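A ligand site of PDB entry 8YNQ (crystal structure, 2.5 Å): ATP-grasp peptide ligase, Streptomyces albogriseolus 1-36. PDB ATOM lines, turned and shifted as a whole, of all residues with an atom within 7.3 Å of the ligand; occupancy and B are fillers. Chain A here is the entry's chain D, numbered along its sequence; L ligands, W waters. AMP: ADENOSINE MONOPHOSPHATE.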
ATOM      1  N   THR A  33     -13.822   0.812 -16.287  1.00  0.00           N
ATOM      2  CA  THR A  33     -13.873  -0.545 -16.817  1.00  0.00           C
ATOM      3  C   THR A  33     -14.108  -0.608 -18.315  1.00  0.00           C
ATOM      4  O   THR A  33     -13.860  -1.645 -18.927  1.00  0.00           O
ATOM      5  CB  THR A  33     -15.008  -1.343 -16.138  1.00  0.00           C
ATOM      6  OG1 THR A  33     -15.133  -0.934 -14.763  1.00  0.00           O
ATOM      7  CG2 THR A  33     -14.682  -2.835 -16.179  1.00  0.00           C
ATOM      8  N   THR A  34     -14.584   0.477 -18.927  1.00  0.00           N
ATOM      9  CA  THR A  34     -14.837   0.507 -20.360  1.00  0.00           C
ATOM     10  C   THR A  34     -13.673   1.096 -21.145  1.00  0.00           C
ATOM     11  O   THR A  34     -13.411   0.661 -22.272  1.00  0.00           O
ATOM     12  CB  THR A  34     -16.112   1.312 -20.659  1.00  0.00           C
ATOM     13  OG1 THR A  34     -17.242   0.606 -20.142  1.00  0.00           O
ATOM     14  CG2 THR A  34     -16.321   1.491 -22.159  1.00  0.00           C
ATOM     15  N   PHE A  37     -11.534  -0.676 -23.973  1.00  0.00           N
ATOM     16  CA  PHE A  37     -11.840  -0.820 -25.400  1.00  0.00           C
ATOM     17  C   PHE A  37     -11.287   0.328 -26.219  1.00  0.00           C
ATOM     18  O   PHE A  37     -11.360   0.282 -27.453  1.00  0.00           O
ATOM     19  CB  PHE A  37     -13.349  -0.973 -25.583  1.00  0.00           C
ATOM     20  CG  PHE A  37     -13.930  -2.060 -24.710  1.00  0.00           C
ATOM     21  CD1 PHE A  37     -13.621  -3.385 -24.939  1.00  0.00           C
ATOM     22  CD2 PHE A  37     -14.736  -1.750 -23.626  1.00  0.00           C
ATOM     23  CE1 PHE A  37     -14.102  -4.382 -24.130  1.00  0.00           C
ATOM     24  CE2 PHE A  37     -15.238  -2.737 -22.817  1.00  0.00           C
ATOM     25  CZ  PHE A  37     -14.919  -4.065 -23.067  1.00  0.00           C
ATOM     26  N   LEU A  47     -15.040   6.194 -29.420  1.00  0.00           N
ATOM     27  CA  LEU A  47     -15.406   5.250 -28.398  1.00  0.00           C
ATOM     28  C   LEU A  47     -16.620   5.808 -27.672  1.00  0.00           C
ATOM     29  O   LEU A  47     -16.784   7.021 -27.565  1.00  0.00           O
ATOM     30  CB  LEU A  47     -14.267   5.004 -27.410  1.00  0.00           C
ATOM     31  CG  LEU A  47     -14.572   4.051 -26.253  1.00  0.00           C
ATOM     32  CD1 LEU A  47     -14.967   2.620 -26.768  1.00  0.00           C
ATOM     33  CD2 LEU A  47     -13.397   4.005 -25.278  1.00  0.00           C
ATOM     34  N   VAL A  48     -17.467   4.910 -27.202  1.00  0.00           N
ATOM     35  CA  VAL A  48     -18.567   5.254 -26.316  1.00  0.00           C
ATOM     36  C   VAL A  48     -18.306   4.557 -24.982  1.00  0.00           C
ATOM     37  O   VAL A  48     -17.983   3.364 -24.962  1.00  0.00           O
ATOM     38  CB  VAL A  48     -19.930   4.844 -26.882  1.00  0.00           C
ATOM     39  CG1 VAL A  48     -20.993   5.178 -25.898  1.00  0.00           C
ATOM     40  CG2 VAL A  48     -20.171   5.543 -28.202  1.00  0.00           C
ATOM     41  N   ILE A  49     -18.403   5.314 -23.896  1.00  0.00           N
ATOM     42  CA  ILE A  49     -18.201   4.763 -22.563  1.00  0.00           C
ATOM     43  C   ILE A  49     -19.318   5.259 -21.659  1.00  0.00           C
ATOM     44  O   ILE A  49     -19.798   6.393 -21.806  1.00  0.00           O
ATOM     45  CB  ILE A  49     -16.832   5.136 -21.975  1.00  0.00           C
ATOM     46  CG1 ILE A  49     -16.914   6.386 -21.086  1.00  0.00           C
ATOM     47  CG2 ILE A  49     -15.809   5.331 -23.082  1.00  0.00           C
ATOM     48  CD1 ILE A  49     -15.560   7.065 -20.826  1.00  0.00           C
ATOM     49  N   PRO A  50     -19.798   4.430 -20.740  1.00  0.00           N
ATOM     50  CA  PRO A  50     -20.621   4.916 -19.621  1.00  0.00           C
ATOM     51  C   PRO A  50     -19.795   5.291 -18.399  1.00  0.00           C
ATOM     52  O   PRO A  50     -20.377   5.771 -17.419  1.00  0.00           O
ATOM     53  CB  PRO A  50     -21.503   3.703 -19.328  1.00  0.00           C
ATOM     54  CG  PRO A  50     -20.592   2.535 -19.590  1.00  0.00           C
ATOM     55  CD  PRO A  50     -19.631   2.965 -20.696  1.00  0.00           C
ATOM     56  N   ASP A  51     -18.477   5.087 -18.452  1.00  0.00           N
ATOM     57  CA  ASP A  51     -17.518   5.253 -17.370  1.00  0.00           C
ATOM     58  C   ASP A  51     -16.869   6.649 -17.452  1.00  0.00           C
ATOM     59  O   ASP A  51     -17.442   7.574 -18.041  1.00  0.00           O
ATOM     60  CB  ASP A  51     -16.458   4.131 -17.458  1.00  0.00           C
ATOM     61  CG  ASP A  51     -17.033   2.739 -17.162  1.00  0.00           C
ATOM     62  OD1 ASP A  51     -18.236   2.513 -17.451  1.00  0.00           O
ATOM     63  OD2 ASP A  51     -16.300   1.854 -16.662  1.00  0.00           O
ATOM     64  N   PRO A  80     -26.069   3.695 -18.498  1.00  0.00           N
ATOM     65  CA  PRO A  80     -25.484   2.539 -19.170  1.00  0.00           C
ATOM     66  C   PRO A  80     -25.872   2.489 -20.638  1.00  0.00           C
ATOM     67  O   PRO A  80     -26.857   3.083 -21.072  1.00  0.00           O
ATOM     68  CB  PRO A  80     -26.038   1.345 -18.396  1.00  0.00           C
ATOM     69  CG  PRO A  80     -26.644   1.911 -17.144  1.00  0.00           C
ATOM     70  CD  PRO A  80     -27.043   3.304 -17.468  1.00  0.00           C
ATOM     71  N   LEU A  81     -25.055   1.770 -21.413  1.00  0.00           N
ATOM     72  CA  LEU A  81     -25.175   1.691 -22.874  1.00  0.00           C
ATOM     73  C   LEU A  81     -26.175   0.616 -23.236  1.00  0.00           C
ATOM     74  O   LEU A  81     -25.807  -0.509 -23.537  1.00  0.00           O
ATOM     75  CB  LEU A  81     -23.822   1.362 -23.492  1.00  0.00           C
ATOM     76  CG  LEU A  81     -22.817   2.503 -23.479  1.00  0.00           C
ATOM     77  CD1 LEU A  81     -21.569   2.125 -24.275  1.00  0.00           C
ATOM     78  CD2 LEU A  81     -23.494   3.765 -24.023  1.00  0.00           C
ATOM     79  N   SER A  82     -27.463   0.969 -23.252  1.00  0.00           N
ATOM     80  CA  SER A  82     -28.512  -0.037 -23.383  1.00  0.00           C
ATOM     81  C   SER A  82     -29.293   0.155 -24.682  1.00  0.00           C
ATOM     82  O   SER A  82     -29.042   1.089 -25.454  1.00  0.00           O
ATOM     83  CB  SER A  82     -29.469   0.007 -22.198  1.00  0.00           C
ATOM     84  OG  SER A  82     -30.393   1.046 -22.405  1.00  0.00           O
ATOM     85  N   GLU A  83     -30.260  -0.746 -24.896  1.00  0.00           N
ATOM     86  CA  GLU A  83     -31.109  -0.616 -26.066  1.00  0.00           C
ATOM     87  C   GLU A  83     -31.786   0.747 -26.120  1.00  0.00           C
ATOM     88  O   GLU A  83     -31.839   1.382 -27.183  1.00  0.00           O
ATOM     89  CB  GLU A  83     -32.155  -1.740 -26.071  1.00  0.00           C
ATOM     90  CG  GLU A  83     -31.588  -3.139 -25.930  1.00  0.00           C
ATOM     91  CD  GLU A  83     -31.594  -3.860 -27.234  1.00  0.00           C
ATOM     92  OE1 GLU A  83     -31.304  -3.186 -28.239  1.00  0.00           O
ATOM     93  OE2 GLU A  83     -31.884  -5.075 -27.283  1.00  0.00           O
ATOM     94  N   LEU A  86     -29.476   3.323 -27.475  1.00  0.00           N
ATOM     95  CA  LEU A  86     -29.218   3.145 -28.900  1.00  0.00           C
ATOM     96  C   LEU A  86     -30.354   3.658 -29.740  1.00  0.00           C
ATOM     97  O   LEU A  86     -30.130   4.174 -30.842  1.00  0.00           O
ATOM     98  CB  LEU A  86     -28.965   1.666 -29.192  1.00  0.00           C
ATOM     99  CG  LEU A  86     -27.754   1.004 -28.528  1.00  0.00           C
ATOM    100  CD1 LEU A  86     -27.399  -0.259 -29.310  1.00  0.00           C
ATOM    101  CD2 LEU A  86     -26.545   1.949 -28.418  1.00  0.00           C
ATOM    102  N   LEU A 107     -19.992   0.795 -37.694  1.00  0.00           N
ATOM    103  CA  LEU A 107     -20.258   0.654 -36.265  1.00  0.00           C
ATOM    104  C   LEU A 107     -19.593  -0.626 -35.759  1.00  0.00           C
ATOM    105  O   LEU A 107     -19.540  -1.624 -36.488  1.00  0.00           O
ATOM    106  CB  LEU A 107     -21.763   0.649 -35.996  1.00  0.00           C
ATOM    107  CG  LEU A 107     -22.358   0.375 -34.607  1.00  0.00           C
ATOM    108  CD1 LEU A 107     -22.123   1.520 -33.619  1.00  0.00           C
ATOM    109  CD2 LEU A 107     -23.837   0.116 -34.793  1.00  0.00           C
ATOM    110  N   PHE A 108     -19.067  -0.599 -34.537  1.00  0.00           N
ATOM    111  CA  PHE A 108     -18.245  -1.690 -33.994  1.00  0.00           C
ATOM    112  C   PHE A 108     -18.831  -2.179 -32.684  1.00  0.00           C
ATOM    113  O   PHE A 108     -18.247  -1.980 -31.614  1.00  0.00           O
ATOM    114  CB  PHE A 108     -16.790  -1.243 -33.812  1.00  0.00           C
ATOM    115  CG  PHE A 108     -15.836  -2.350 -33.409  1.00  0.00           C
ATOM    116  CD1 PHE A 108     -15.551  -3.402 -34.261  1.00  0.00           C
ATOM    117  CD2 PHE A 108     -15.196  -2.322 -32.178  1.00  0.00           C
ATOM    118  CE1 PHE A 108     -14.655  -4.395 -33.900  1.00  0.00           C
ATOM    119  CE2 PHE A 108     -14.288  -3.320 -31.806  1.00  0.00           C
ATOM    120  CZ  PHE A 108     -14.029  -4.354 -32.657  1.00  0.00           C
ATOM    121  N   PRO A 109     -19.975  -2.846 -32.726  1.00  0.00           N
ATOM    122  CA  PRO A 109     -20.704  -3.143 -31.492  1.00  0.00           C
ATOM    123  C   PRO A 109     -20.169  -4.387 -30.788  1.00  0.00           C
ATOM    124  O   PRO A 109     -19.623  -5.298 -31.398  1.00  0.00           O
ATOM    125  CB  PRO A 109     -22.137  -3.361 -31.985  1.00  0.00           C
ATOM    126  CG  PRO A 109     -21.934  -3.929 -33.348  1.00  0.00           C
ATOM    127  CD  PRO A 109     -20.723  -3.265 -33.926  1.00  0.00           C
ATOM    128  N   CYS A 110     -20.323  -4.395 -29.470  1.00  0.00           N
ATOM    129  CA  CYS A 110     -19.906  -5.550 -28.699  1.00  0.00           C
ATOM    130  C   CYS A 110     -20.887  -6.694 -28.835  1.00  0.00           C
ATOM    131  O   CYS A 110     -20.486  -7.858 -28.836  1.00  0.00           O
ATOM    132  CB  CYS A 110     -19.749  -5.183 -27.225  1.00  0.00           C
ATOM    133  SG  CYS A 110     -19.639  -6.588 -26.081  1.00  0.00           S
ATOM    134  N   VAL A 111     -22.178  -6.371 -28.923  1.00  0.00           N
ATOM    135  CA  VAL A 111     -23.248  -7.364 -28.990  1.00  0.00           C
ATOM    136  C   VAL A 111     -24.116  -6.961 -30.173  1.00  0.00           C
ATOM    137  O   VAL A 111     -24.795  -5.926 -30.118  1.00  0.00           O
ATOM    138  CB  VAL A 111     -24.075  -7.424 -27.697  1.00  0.00           C
ATOM    139  CG1 VAL A 111     -24.771  -8.761 -27.575  1.00  0.00           C
ATOM    140  CG2 VAL A 111     -23.197  -7.189 -26.473  1.00  0.00           C
ATOM    141  N   SER A 112     -24.105  -7.752 -31.241  1.00  0.00           N
ATOM    142  CA  SER A 112     -24.747  -7.252 -32.453  1.00  0.00           C
ATOM    143  C   SER A 112     -26.269  -7.327 -32.343  1.00  0.00           C
ATOM    144  O   SER A 112     -26.923  -8.129 -33.023  1.00  0.00           O
ATOM    145  CB  SER A 112     -24.199  -8.001 -33.670  1.00  0.00           C
ATOM    146  OG  SER A 112     -22.804  -7.720 -33.860  1.00  0.00           O
ATOM    147  N   THR A 113     -26.834  -6.449 -31.513  1.00  0.00           N
ATOM    148  CA  THR A 113     -28.232  -6.384 -31.113  1.00  0.00           C
ATOM    149  C   THR A 113     -29.114  -5.797 -32.215  1.00  0.00           C
ATOM    150  O   THR A 113     -28.649  -5.170 -33.172  1.00  0.00           O
ATOM    151  CB  THR A 113     -28.411  -5.507 -29.881  1.00  0.00           C
ATOM    152  OG1 THR A 113     -27.990  -4.161 -30.195  1.00  0.00           O
ATOM    153  CG2 THR A 113     -27.597  -6.038 -28.744  1.00  0.00           C
ATOM    154  N   ALA A 115     -31.041  -3.194 -31.813  1.00  0.00           N
ATOM    155  CA  ALA A 115     -30.876  -1.734 -31.823  1.00  0.00           C
ATOM    156  C   ALA A 115     -29.596  -1.344 -32.549  1.00  0.00           C
ATOM    157  O   ALA A 115     -29.558  -0.300 -33.221  1.00  0.00           O
ATOM    158  CB  ALA A 115     -30.871  -1.173 -30.406  1.00  0.00           C
ATOM    159  N   ALA A 116     -28.550  -2.167 -32.441  1.00  0.00           N
ATOM    160  CA  ALA A 116     -27.284  -1.862 -33.098  1.00  0.00           C
ATOM    161  C   ALA A 116     -27.413  -1.901 -34.613  1.00  0.00           C
ATOM    162  O   ALA A 116     -26.793  -1.105 -35.318  1.00  0.00           O
ATOM    163  CB  ALA A 116     -26.214  -2.845 -32.630  1.00  0.00           C
ATOM    164  N   ARG A 342     -20.383 -12.463 -28.892  1.00  0.00           N
ATOM    165  CA  ARG A 342     -19.980 -11.134 -28.435  1.00  0.00           C
ATOM    166  C   ARG A 342     -18.460 -11.176 -28.273  1.00  0.00           C
ATOM    167  O   ARG A 342     -17.833 -12.219 -28.486  1.00  0.00           O
ATOM    168  CB  ARG A 342     -20.728 -10.738 -27.160  1.00  0.00           C
ATOM    169  CG  ARG A 342     -20.616 -11.730 -25.985  1.00  0.00           C
ATOM    170  CD  ARG A 342     -19.500 -11.306 -25.005  1.00  0.00           C
ATOM    171  NE  ARG A 342     -19.433 -11.977 -23.697  1.00  0.00           N
ATOM    172  CZ  ARG A 342     -18.566 -12.926 -23.350  1.00  0.00           C
ATOM    173  NH1 ARG A 342     -17.724 -13.456 -24.225  1.00  0.00           N
ATOM    174  NH2 ARG A 342     -18.548 -13.371 -22.092  1.00  0.00           N
ATOM    175  N   TRP A 343     -17.865 -10.026 -27.927  1.00  0.00           N
ATOM    176  CA  TRP A 343     -16.426  -9.979 -27.659  1.00  0.00           C
ATOM    177  C   TRP A 343     -16.115 -10.886 -26.490  1.00  0.00           C
ATOM    178  O   TRP A 343     -16.719 -10.748 -25.419  1.00  0.00           O
ATOM    179  CB  TRP A 343     -15.964  -8.558 -27.335  1.00  0.00           C
ATOM    180  CG  TRP A 343     -16.240  -7.496 -28.392  1.00  0.00           C
ATOM    181  CD1 TRP A 343     -16.405  -7.690 -29.746  1.00  0.00           C
ATOM    182  CD2 TRP A 343     -16.362  -6.081 -28.180  1.00  0.00           C
ATOM    183  NE1 TRP A 343     -16.624  -6.485 -30.375  1.00  0.00           N
ATOM    184  CE2 TRP A 343     -16.598  -5.490 -29.434  1.00  0.00           C
ATOM    185  CE3 TRP A 343     -16.308  -5.272 -27.043  1.00  0.00           C
ATOM    186  CZ2 TRP A 343     -16.778  -4.113 -29.578  1.00  0.00           C
ATOM    187  CZ3 TRP A 343     -16.465  -3.899 -27.205  1.00  0.00           C
ATOM    188  CH2 TRP A 343     -16.705  -3.338 -28.458  1.00  0.00           C
HETATM  189  P   AMP L   1     -23.015  -3.289 -27.720  1.00  0.00           P
HETATM  190  O1P AMP L   1     -22.516  -4.213 -26.628  1.00  0.00           O
HETATM  191  O2P AMP L   1     -24.446  -2.840 -27.482  1.00  0.00           O
HETATM  192  O3P AMP L   1     -22.774  -3.820 -29.119  1.00  0.00           O
HETATM  193  O5' AMP L   1     -22.118  -1.956 -27.567  1.00  0.00           O
HETATM  194  C5' AMP L   1     -20.689  -1.991 -27.523  1.00  0.00           C
HETATM  195  C4' AMP L   1     -20.110  -0.948 -26.579  1.00  0.00           C
HETATM  196  O4' AMP L   1     -21.128  -0.585 -25.632  1.00  0.00           O
HETATM  197  C3' AMP L   1     -18.913  -1.346 -25.749  1.00  0.00           C
HETATM  198  O3' AMP L   1     -18.188  -0.170 -25.385  1.00  0.00           O
HETATM  199  C2' AMP L   1     -19.545  -1.956 -24.491  1.00  0.00           C
HETATM  200  O2' AMP L   1     -18.825  -1.703 -23.299  1.00  0.00           O
HETATM  201  C1' AMP L   1     -20.940  -1.310 -24.434  1.00  0.00           C
HETATM  202  N9  AMP L   1     -22.062  -2.241 -24.314  1.00  0.00           N
HETATM  203  C8  AMP L   1     -23.256  -2.006 -24.894  1.00  0.00           C
HETATM  204  N7  AMP L   1     -24.145  -2.998 -24.646  1.00  0.00           N
HETATM  205  C5  AMP L   1     -23.537  -3.896 -23.855  1.00  0.00           C
HETATM  206  C6  AMP L   1     -23.933  -5.153 -23.197  1.00  0.00           C
HETATM  207  N6  AMP L   1     -25.194  -5.637 -23.367  1.00  0.00           N
HETATM  208  N1  AMP L   1     -23.012  -5.802 -22.453  1.00  0.00           N
HETATM  209  C2  AMP L   1     -21.766  -5.315 -22.285  1.00  0.00           C
HETATM  210  N3  AMP L   1     -21.335  -4.176 -22.832  1.00  0.00           N
HETATM  211  C4  AMP L   1     -22.162  -3.404 -23.622  1.00  0.00           C
HETATM  212  O   HOH W   1     -19.039  -5.160 -22.819  1.00  0.00           O
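Water W1 lies within hydrogen-bond range of N3 of the ligand (2.5 Å) and SG of Cys 110 (3.6 Å).
The backbone NH (N) of Cys 110 lies within hydrogen-bond range of an oxygen (O3P) of the ligand, 2.5 Å away. N of Val 111 is in hydrogen-bond range of O3P of the ligand (2.6 Å). SG of Cys 110 sits close to O1P of the ligand (3.8 Å). O3P of the ligand sits close to O of Val 111, at 3.1 Å.
O of Leu 81 lies close to N7 of the ligand (3.2 Å). Merely in contact with the ligand: Pro 109 (3.0 Å), Val 48 (3.6 Å), Phe 37 (3.8 Å) and Trp 343 (3.8 Å). Hydrophobic or aromatic side chains that line the ligand: Phe 37, Leu 81, Pro 109, Val 111 and Trp 343. The nearest printed residue that does not touch the ligand is Thr 34 (4.1 Å).
O of Pro 109 sits at hydrogen-bond distance from NE1 of Trp 343.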
